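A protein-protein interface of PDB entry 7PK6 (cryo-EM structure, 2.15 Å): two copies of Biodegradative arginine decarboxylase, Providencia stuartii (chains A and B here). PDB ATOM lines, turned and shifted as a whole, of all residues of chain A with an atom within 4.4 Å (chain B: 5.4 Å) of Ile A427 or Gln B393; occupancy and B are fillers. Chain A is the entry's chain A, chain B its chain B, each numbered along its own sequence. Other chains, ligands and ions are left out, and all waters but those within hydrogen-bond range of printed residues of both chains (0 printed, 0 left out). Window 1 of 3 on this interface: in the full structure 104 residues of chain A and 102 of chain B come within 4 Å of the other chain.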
ATOM      1  N   VAL A 227     -17.704 -13.713  15.101  1.00  0.00           N
ATOM      2  CA  VAL A 227     -18.575 -12.559  14.919  1.00  0.00           C
ATOM      3  C   VAL A 227     -18.668 -12.144  13.458  1.00  0.00           C
ATOM      4  O   VAL A 227     -19.182 -11.066  13.157  1.00  0.00           O
ATOM      5  CB  VAL A 227     -18.136 -11.374  15.798  1.00  0.00           C
ATOM      6  CG1 VAL A 227     -18.320 -11.705  17.260  1.00  0.00           C
ATOM      7  CG2 VAL A 227     -16.696 -10.988  15.507  1.00  0.00           C
ATOM      8  N   SER A 392     -27.618 -11.841  14.119  1.00  0.00           N
ATOM      9  CA  SER A 392     -26.888 -12.042  12.875  1.00  0.00           C
ATOM     10  C   SER A 392     -25.392 -11.858  13.097  1.00  0.00           C
ATOM     11  O   SER A 392     -24.958 -11.056  13.928  1.00  0.00           O
ATOM     12  CB  SER A 392     -27.376 -11.067  11.805  1.00  0.00           C
ATOM     13  OG  SER A 392     -28.678 -11.394  11.368  1.00  0.00           O
ATOM     14  N   GLN A 393     -24.608 -12.628  12.344  1.00  0.00           N
ATOM     15  CA  GLN A 393     -23.147 -12.720  12.342  1.00  0.00           C
ATOM     16  C   GLN A 393     -22.608 -13.581  13.481  1.00  0.00           C
ATOM     17  O   GLN A 393     -21.399 -13.794  13.534  1.00  0.00           O
ATOM     18  CB  GLN A 393     -22.443 -11.351  12.390  1.00  0.00           C
ATOM     19  CG  GLN A 393     -22.829 -10.407  11.268  1.00  0.00           C
ATOM     20  CD  GLN A 393     -22.056  -9.103  11.290  1.00  0.00           C
ATOM     21  OE1 GLN A 393     -22.590  -8.053  10.954  1.00  0.00           O
ATOM     22  NE2 GLN A 393     -20.790  -9.167  11.677  1.00  0.00           N
ATOM     23  N   ALA A 394     -23.448 -14.090  14.376  1.00  0.00           N
ATOM     24  CA  ALA A 394     -22.980 -15.001  15.411  1.00  0.00           C
ATOM     25  C   ALA A 394     -22.813 -16.402  14.841  1.00  0.00           C
ATOM     26  O   ALA A 394     -23.677 -16.900  14.117  1.00  0.00           O
ATOM     27  CB  ALA A 394     -23.946 -15.024  16.592  1.00  0.00           C
ATOM     28  N   THR A 420     -11.874  -9.613  13.446  1.00  0.00           N
ATOM     29  CA  THR A 420     -11.643  -8.190  13.625  1.00  0.00           C
ATOM     30  C   THR A 420     -11.051  -7.952  15.005  1.00  0.00           C
ATOM     31  O   THR A 420     -11.304  -8.708  15.945  1.00  0.00           O
ATOM     32  CB  THR A 420     -12.938  -7.375  13.463  1.00  0.00           C
ATOM     33  OG1 THR A 420     -12.709  -6.022  13.868  1.00  0.00           O
ATOM     34  CG2 THR A 420     -14.052  -7.960  14.310  1.00  0.00           C
ATOM     35  N   SER A 422     -11.805  -5.496  16.904  1.00  0.00           N
ATOM     36  CA  SER A 422     -12.805  -4.844  17.749  1.00  0.00           C
ATOM     37  C   SER A 422     -14.148  -5.541  17.591  1.00  0.00           C
ATOM     38  O   SER A 422     -15.074  -4.996  16.979  1.00  0.00           O
ATOM     39  CB  SER A 422     -12.928  -3.360  17.409  1.00  0.00           C
ATOM     40  OG  SER A 422     -11.659  -2.774  17.194  1.00  0.00           O
ATOM     41  N   PRO A 423     -14.296  -6.744  18.139  1.00  0.00           N
ATOM     42  CA  PRO A 423     -15.587  -7.432  18.053  1.00  0.00           C
ATOM     43  C   PRO A 423     -16.664  -6.721  18.855  1.00  0.00           C
ATOM     44  O   PRO A 423     -16.402  -6.111  19.892  1.00  0.00           O
ATOM     45  CB  PRO A 423     -15.288  -8.817  18.635  1.00  0.00           C
ATOM     46  CG  PRO A 423     -14.119  -8.602  19.515  1.00  0.00           C
ATOM     47  CD  PRO A 423     -13.295  -7.545  18.861  1.00  0.00           C
ATOM     48  N   LEU A 424     -17.890  -6.806  18.354  1.00  0.00           N
ATOM     49  CA  LEU A 424     -19.048  -6.300  19.077  1.00  0.00           C
ATOM     50  C   LEU A 424     -19.508  -7.359  20.071  1.00  0.00           C
ATOM     51  O   LEU A 424     -19.919  -8.452  19.674  1.00  0.00           O
ATOM     52  CB  LEU A 424     -20.167  -5.935  18.108  1.00  0.00           C
ATOM     53  CG  LEU A 424     -21.405  -5.289  18.728  1.00  0.00           C
ATOM     54  CD1 LEU A 424     -21.047  -3.969  19.387  1.00  0.00           C
ATOM     55  CD2 LEU A 424     -22.492  -5.099  17.690  1.00  0.00           C
ATOM     56  N   TYR A 425     -19.436  -7.036  21.361  1.00  0.00           N
ATOM     57  CA  TYR A 425     -19.671  -8.031  22.398  1.00  0.00           C
ATOM     58  C   TYR A 425     -21.129  -8.458  22.493  1.00  0.00           C
ATOM     59  O   TYR A 425     -21.412  -9.498  23.091  1.00  0.00           O
ATOM     60  CB  TYR A 425     -19.193  -7.504  23.750  1.00  0.00           C
ATOM     61  CG  TYR A 425     -17.696  -7.590  23.932  1.00  0.00           C
ATOM     62  CD1 TYR A 425     -16.885  -8.078  22.919  1.00  0.00           C
ATOM     63  CD2 TYR A 425     -17.095  -7.186  25.111  1.00  0.00           C
ATOM     64  CE1 TYR A 425     -15.523  -8.160  23.075  1.00  0.00           C
ATOM     65  CE2 TYR A 425     -15.732  -7.265  25.278  1.00  0.00           C
ATOM     66  CZ  TYR A 425     -14.950  -7.750  24.256  1.00  0.00           C
ATOM     67  OH  TYR A 425     -13.592  -7.836  24.415  1.00  0.00           O
ATOM     68  N   ALA A 426     -22.055  -7.688  21.922  1.00  0.00           N
ATOM     69  CA  ALA A 426     -23.445  -8.124  21.878  1.00  0.00           C
ATOM     70  C   ALA A 426     -23.607  -9.397  21.053  1.00  0.00           C
ATOM     71  O   ALA A 426     -24.413 -10.264  21.404  1.00  0.00           O
ATOM     72  CB  ALA A 426     -24.329  -7.007  21.323  1.00  0.00           C
ATOM     73  N   ILE A 427     -22.849  -9.529  19.964  1.00  0.00           N
ATOM     74  CA  ILE A 427     -22.908 -10.738  19.148  1.00  0.00           C
ATOM     75  C   ILE A 427     -22.410 -11.947  19.936  1.00  0.00           C
ATOM     76  O   ILE A 427     -23.028 -13.020  19.916  1.00  0.00           O
ATOM     77  CB  ILE A 427     -22.111 -10.536  17.847  1.00  0.00           C
ATOM     78  CG1 ILE A 427     -22.696  -9.378  17.040  1.00  0.00           C
ATOM     79  CG2 ILE A 427     -22.097 -11.807  17.021  1.00  0.00           C
ATOM     80  CD1 ILE A 427     -21.850  -8.964  15.858  1.00  0.00           C
ATOM     81  N   CYS A 428     -21.290 -11.794  20.643  1.00  0.00           N
ATOM     82  CA  CYS A 428     -20.776 -12.890  21.461  1.00  0.00           C
ATOM     83  C   CYS A 428     -21.737 -13.232  22.592  1.00  0.00           C
ATOM     84  O   CYS A 428     -21.894 -14.404  22.949  1.00  0.00           O
ATOM     85  CB  CYS A 428     -19.396 -12.535  22.015  1.00  0.00           C
ATOM     86  SG  CYS A 428     -18.327 -11.639  20.876  1.00  0.00           S
ATOM     87  N   ALA A 429     -22.383 -12.220  23.171  1.00  0.00           N
ATOM     88  CA  ALA A 429     -23.375 -12.470  24.209  1.00  0.00           C
ATOM     89  C   ALA A 429     -24.567 -13.244  23.659  1.00  0.00           C
ATOM     90  O   ALA A 429     -25.113 -14.115  24.342  1.00  0.00           O
ATOM     91  CB  ALA A 429     -23.829 -11.151  24.829  1.00  0.00           C
ATOM     92  N   SER A 430     -24.996 -12.927  22.436  1.00  0.00           N
ATOM     93  CA  SER A 430     -26.075 -13.690  21.819  1.00  0.00           C
ATOM     94  C   SER A 430     -25.651 -15.133  21.560  1.00  0.00           C
ATOM     95  O   SER A 430     -26.445 -16.060  21.747  1.00  0.00           O
ATOM     96  CB  SER A 430     -26.541 -13.009  20.530  1.00  0.00           C
ATOM     97  OG  SER A 430     -25.722 -13.342  19.430  1.00  0.00           O
ATOM     98  N   ASN A 431     -24.400 -15.342  21.144  1.00  0.00           N
ATOM     99  CA  ASN A 431     -23.886 -16.705  21.004  1.00  0.00           C
ATOM    100  C   ASN A 431     -23.946 -17.456  22.330  1.00  0.00           C
ATOM    101  O   ASN A 431     -24.365 -18.621  22.388  1.00  0.00           O
ATOM    102  CB  ASN A 431     -22.449 -16.667  20.484  1.00  0.00           C
ATOM    103  CG  ASN A 431     -22.295 -17.336  19.139  1.00  0.00           C
ATOM    104  OD1 ASN A 431     -23.262 -17.800  18.554  1.00  0.00           O
ATOM    105  ND2 ASN A 431     -21.070 -17.390  18.645  1.00  0.00           N
ATOM    106  N   VAL B 226     -18.888  -1.601   6.080  1.00  0.00           N
ATOM    107  CA  VAL B 226     -18.268  -2.872   6.433  1.00  0.00           C
ATOM    108  C   VAL B 226     -18.677  -3.228   7.855  1.00  0.00           C
ATOM    109  O   VAL B 226     -18.722  -2.358   8.730  1.00  0.00           O
ATOM    110  CB  VAL B 226     -16.731  -2.801   6.291  1.00  0.00           C
ATOM    111  CG1 VAL B 226     -16.056  -3.994   6.941  1.00  0.00           C
ATOM    112  CG2 VAL B 226     -16.342  -2.703   4.827  1.00  0.00           C
ATOM    113  N   VAL B 227     -18.989  -4.500   8.085  1.00  0.00           N
ATOM    114  CA  VAL B 227     -19.406  -4.979   9.396  1.00  0.00           C
ATOM    115  C   VAL B 227     -18.364  -5.892  10.024  1.00  0.00           C
ATOM    116  O   VAL B 227     -18.648  -6.551  11.026  1.00  0.00           O
ATOM    117  CB  VAL B 227     -20.778  -5.672   9.336  1.00  0.00           C
ATOM    118  CG1 VAL B 227     -21.858  -4.677   8.983  1.00  0.00           C
ATOM    119  CG2 VAL B 227     -20.759  -6.825   8.346  1.00  0.00           C
ATOM    120  N   VAL B 228     -17.161  -5.945   9.461  1.00  0.00           N
ATOM    121  CA  VAL B 228     -16.059  -6.715  10.018  1.00  0.00           C
ATOM    122  C   VAL B 228     -14.908  -5.799  10.433  1.00  0.00           C
ATOM    123  O   VAL B 228     -13.770  -6.232  10.546  1.00  0.00           O
ATOM    124  CB  VAL B 228     -15.595  -7.805   9.031  1.00  0.00           C
ATOM    125  CG1 VAL B 228     -14.820  -8.900   9.745  1.00  0.00           C
ATOM    126  CG2 VAL B 228     -16.780  -8.398   8.299  1.00  0.00           C
ATOM    127  N   GLY B 229     -15.197  -4.526  10.649  1.00  0.00           N
ATOM    128  CA  GLY B 229     -14.195  -3.590  11.110  1.00  0.00           C
ATOM    129  C   GLY B 229     -13.192  -3.204  10.037  1.00  0.00           C
ATOM    130  O   GLY B 229     -13.255  -3.608   8.873  1.00  0.00           O
ATOM    131  N   HIS B 385     -16.056   3.107  14.763  1.00  0.00           N
ATOM    132  CA  HIS B 385     -16.230   2.874  16.212  1.00  0.00           C
ATOM    133  C   HIS B 385     -15.067   3.460  17.010  1.00  0.00           C
ATOM    134  O   HIS B 385     -15.243   3.621  18.193  1.00  0.00           O
ATOM    135  CB  HIS B 385     -16.403   1.385  16.502  1.00  0.00           C
ATOM    136  CG  HIS B 385     -15.273   0.552  16.032  1.00  0.00           C
ATOM    137  ND1 HIS B 385     -14.137   0.371  16.783  1.00  0.00           N
ATOM    138  CD2 HIS B 385     -15.101  -0.141  14.893  1.00  0.00           C
ATOM    139  CE1 HIS B 385     -13.304  -0.388  16.121  1.00  0.00           C
ATOM    140  NE2 HIS B 385     -13.879  -0.727  14.973  1.00  0.00           N
ATOM    141  N1  LLP B 386      -5.782  -0.354  11.317  1.00  0.00           N
ATOM    142  C2  LLP B 386      -5.403   0.411  12.332  1.00  0.00           C
ATOM    143  C2' LLP B 386      -4.317   1.417  12.131  1.00  0.00           C
ATOM    144  C3  LLP B 386      -6.020   0.290  13.569  1.00  0.00           C
ATOM    145  O3  LLP B 386      -5.587   1.100  14.545  1.00  0.00           O
ATOM    146  C4  LLP B 386      -7.051  -0.643  13.754  1.00  0.00           C
ATOM    147  C4' LLP B 386      -7.705  -0.765  15.056  1.00  0.00           C
ATOM    148  C5  LLP B 386      -7.422  -1.439  12.660  1.00  0.00           C
ATOM    149  C6  LLP B 386      -6.760  -1.260  11.480  1.00  0.00           C
ATOM    150  C5' LLP B 386      -8.471  -2.507  12.746  1.00  0.00           C
ATOM    151  OP4 LLP B 386      -9.804  -1.961  12.945  1.00  0.00           O
ATOM    152  P   LLP B 386     -10.970  -2.849  13.545  1.00  0.00           P
ATOM    153  OP1 LLP B 386     -12.194  -2.053  13.276  1.00  0.00           O
ATOM    154  OP2 LLP B 386     -10.964  -4.171  12.843  1.00  0.00           O
ATOM    155  OP3 LLP B 386     -10.609  -2.951  14.972  1.00  0.00           O
ATOM    156  N   LLP B 386     -13.928   3.722  16.382  1.00  0.00           N
ATOM    157  CA  LLP B 386     -12.750   4.184  17.163  1.00  0.00           C
ATOM    158  CB  LLP B 386     -11.413   3.889  16.474  1.00  0.00           C
ATOM    159  CG  LLP B 386     -10.786   2.539  16.798  1.00  0.00           C
ATOM    160  CD  LLP B 386      -9.614   2.164  15.899  1.00  0.00           C
ATOM    161  CE  LLP B 386      -9.481   0.669  15.675  1.00  0.00           C
ATOM    162  NZ  LLP B 386      -8.083   0.249  15.732  1.00  0.00           N
ATOM    163  C   LLP B 386     -12.933   5.636  17.621  1.00  0.00           C
ATOM    164  O   LLP B 386     -13.086   5.831  18.814  1.00  0.00           O
ATOM    165  N   LEU B 391     -20.953   1.564  16.660  1.00  0.00           N
ATOM    166  CA  LEU B 391     -20.719   0.318  17.367  1.00  0.00           C
ATOM    167  C   LEU B 391     -19.471  -0.372  16.833  1.00  0.00           C
ATOM    168  O   LEU B 391     -19.049  -0.157  15.697  1.00  0.00           O
ATOM    169  CB  LEU B 391     -21.921  -0.612  17.230  1.00  0.00           C
ATOM    170  CG  LEU B 391     -23.219  -0.208  17.923  1.00  0.00           C
ATOM    171  CD1 LEU B 391     -24.376  -1.021  17.374  1.00  0.00           C
ATOM    172  CD2 LEU B 391     -23.096  -0.395  19.419  1.00  0.00           C
ATOM    173  N   SER B 392     -18.885  -1.219  17.674  1.00  0.00           N
ATOM    174  CA  SER B 392     -17.732  -2.009  17.266  1.00  0.00           C
ATOM    175  C   SER B 392     -18.050  -2.811  16.010  1.00  0.00           C
ATOM    176  O   SER B 392     -19.184  -3.245  15.794  1.00  0.00           O
ATOM    177  CB  SER B 392     -17.303  -2.952  18.387  1.00  0.00           C
ATOM    178  OG  SER B 392     -16.731  -2.242  19.466  1.00  0.00           O
ATOM    179  N   GLN B 393     -17.026  -2.991  15.177  1.00  0.00           N
ATOM    180  CA  GLN B 393     -17.009  -3.675  13.882  1.00  0.00           C
ATOM    181  C   GLN B 393     -17.556  -2.809  12.751  1.00  0.00           C
ATOM    182  O   GLN B 393     -17.519  -3.250  11.605  1.00  0.00           O
ATOM    183  CB  GLN B 393     -17.771  -5.014  13.884  1.00  0.00           C
ATOM    184  CG  GLN B 393     -17.285  -6.011  14.917  1.00  0.00           C
ATOM    185  CD  GLN B 393     -17.991  -7.350  14.836  1.00  0.00           C
ATOM    186  OE1 GLN B 393     -18.230  -7.994  15.852  1.00  0.00           O
ATOM    187  NE2 GLN B 393     -18.318  -7.779  13.626  1.00  0.00           N
ATOM    188  N   ALA B 394     -18.043  -1.602  13.020  1.00  0.00           N
ATOM    189  CA  ALA B 394     -18.474  -0.712  11.953  1.00  0.00           C
ATOM    190  C   ALA B 394     -17.268  -0.031  11.319  1.00  0.00           C
ATOM    191  O   ALA B 394     -16.373   0.450  12.015  1.00  0.00           O
ATOM    192  CB  ALA B 394     -19.453   0.334  12.478  1.00  0.00           C
ATOM    193  N   SER B 395     -17.249   0.005   9.993  1.00  0.00           N
ATOM    194  CA  SER B 395     -16.107   0.545   9.270  1.00  0.00           C
ATOM    195  C   SER B 395     -16.572   1.034   7.909  1.00  0.00           C
ATOM    196  O   SER B 395     -17.665   0.702   7.447  1.00  0.00           O
ATOM    197  CB  SER B 395     -15.000  -0.503   9.130  1.00  0.00           C
ATOM    198  OG  SER B 395     -13.916  -0.016   8.366  1.00  0.00           O
ATOM    199  N   LEU B 424     -25.324  -7.980  10.551  1.00  0.00           N
ATOM    200  CA  LEU B 424     -26.178  -7.430  11.594  1.00  0.00           C
ATOM    201  C   LEU B 424     -26.475  -5.973  11.264  1.00  0.00           C
ATOM    202  O   LEU B 424     -25.564  -5.143  11.223  1.00  0.00           O
ATOM    203  CB  LEU B 424     -25.508  -7.558  12.957  1.00  0.00           C
ATOM    204  CG  LEU B 424     -26.345  -7.115  14.157  1.00  0.00           C
ATOM    205  CD1 LEU B 424     -27.595  -7.966  14.281  1.00  0.00           C
ATOM    206  CD2 LEU B 424     -25.527  -7.164  15.431  1.00  0.00           C
ATOM    207  N   ILE B 427     -25.193  -2.721  13.180  1.00  0.00           N
ATOM    208  CA  ILE B 427     -23.871  -2.176  12.887  1.00  0.00           C
ATOM    209  C   ILE B 427     -23.936  -1.193  11.721  1.00  0.00           C
ATOM    210  O   ILE B 427     -23.354  -0.102  11.772  1.00  0.00           O
ATOM    211  CB  ILE B 427     -22.876  -3.320  12.616  1.00  0.00           C
ATOM    212  CG1 ILE B 427     -22.766  -4.228  13.839  1.00  0.00           C
ATOM    213  CG2 ILE B 427     -21.516  -2.771  12.235  1.00  0.00           C
ATOM    214  CD1 ILE B 427     -21.984  -5.498  13.593  1.00  0.00           C
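Ile A427 touches just these residues of chain B: Gln B393 and Leu B424. Of chain A, only Val A227 (3.4 Å), Gln A393 (3.4 Å), Thr A420 (3.8 Å), Ser A422 (3.2 Å), Pro A423 (3.5 Å), Leu A424 (2.8 Å) and Ile A427 (3.7 Å) come within 4 Å of Gln B393. Printed residues of chain A within 4 Å of His B385: Ser A422. Of the printed residues of chain A, Ile B427 touches Gln A393 and Leu A424. Ser B395 touches none of the printed residues of chain A. Ala B394 touches none of the printed residues of chain A. The nearest residue of chain B that does not touch Ile A427 is Ile B427 (4.1 Å). The nearest printed residue of chain B that does not touch Gln A393 is Val B228 (5.3 Å).
The backbone carbonyl oxygen (O) of Val A227 sits at hydrogen-bond distance from the side-chain amide nitrogen (NE2) of Gln B393 (3.4 Å). The backbone carbonyl oxygen of Val B227 sits at hydrogen-bond distance from the side-chain amide nitrogen of Gln A393. NE2 of Gln A393 lies close to NE2 of Gln B393, at 3.4 Å. The side-chain amide oxygen (OE1) of Gln A393 lies within hydrogen-bond range of the backbone NH (N) of Leu B424, at 2.8 Å. The side-chain hydroxyl of Thr A420 lies close to the backbone carbonyl oxygen of Val B228. The side-chain hydroxyl of Thr A420 sits close to OP2 of LLP B386 (2.7 Å). OG of Ser A422 lies close to OP3 of LLP B386, at 2.5 Å. The backbone carbonyl oxygen (O) of Ser A422 lies close to the backbone NH (N) of Gln B393. N of Leu A424 lies within hydrogen-bond range of OE1 of Gln B393 (2.8 Å).
Val A227 touches Gln B393, and with the chains exchanged Gln A393 touches Val B227. Gln A393 touches its own counterpart, Gln B393. Gln A393 touches Leu B424, and with the chains exchanged Leu A424 touches Gln B393. Gln A393 touches Ile B427, and with the chains exchanged Ile A427 touches Gln B393. Of the 21 pairs that touch across the chains among the printed residues, 11 have their exchanged pair printed and touching as well.
Among the printed residues, pairs that only touch across the chains: Ser A392 with Leu B424, Gln A393 with Ile B427, Thr A420 with Gly B229, Thr A420 with Gln B393, Ser A422 with His B385, Ser A422 with Ser B392, Pro A423 with Ser B392, Pro A423 with Gln B393, Leu A424 with Ser B392, Leu A424 with Ile B427, Ile A427 with Gln B393 and Ile A427 with Leu B424.
The side-chain amide nitrogen (NE2) of Gln A393 lies within hydrogen-bond range of the backbone carbonyl oxygen (O) of Val A227, 2.9 Å away. The side-chain hydroxyl of Thr A420 sits close to the backbone NH of Ser A422 (3.2 Å). The backbone carbonyl oxygen (O) of Ile A427 is in hydrogen-bond range of the side-chain hydroxyl (OG) of Ser A430, 2.8 Å away. O of Val B227 is in hydrogen-bond range of NE2 of Gln B393 (2.9 Å). The backbone NH (N) of Gly B229 lies within hydrogen-bond range of the backbone carbonyl oxygen (O) of Gln B393 (2.8 Å). A ring nitrogen (NE2) of His B385 lies close to OP1 of LLP B386 (2.7 Å).
Of the 15 printed residues of chain A, 8 touch a printed residue of chain B. Hydrophobic or aromatic side chains of chain A within 4 Å of the printed part of chain B: Val A227, Leu A424 and Ile A427. Hydrophobic or aromatic side chains of chain B within 4 Å of the printed part of chain A: Val B227, His B385, Leu B424 and Ile B427.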
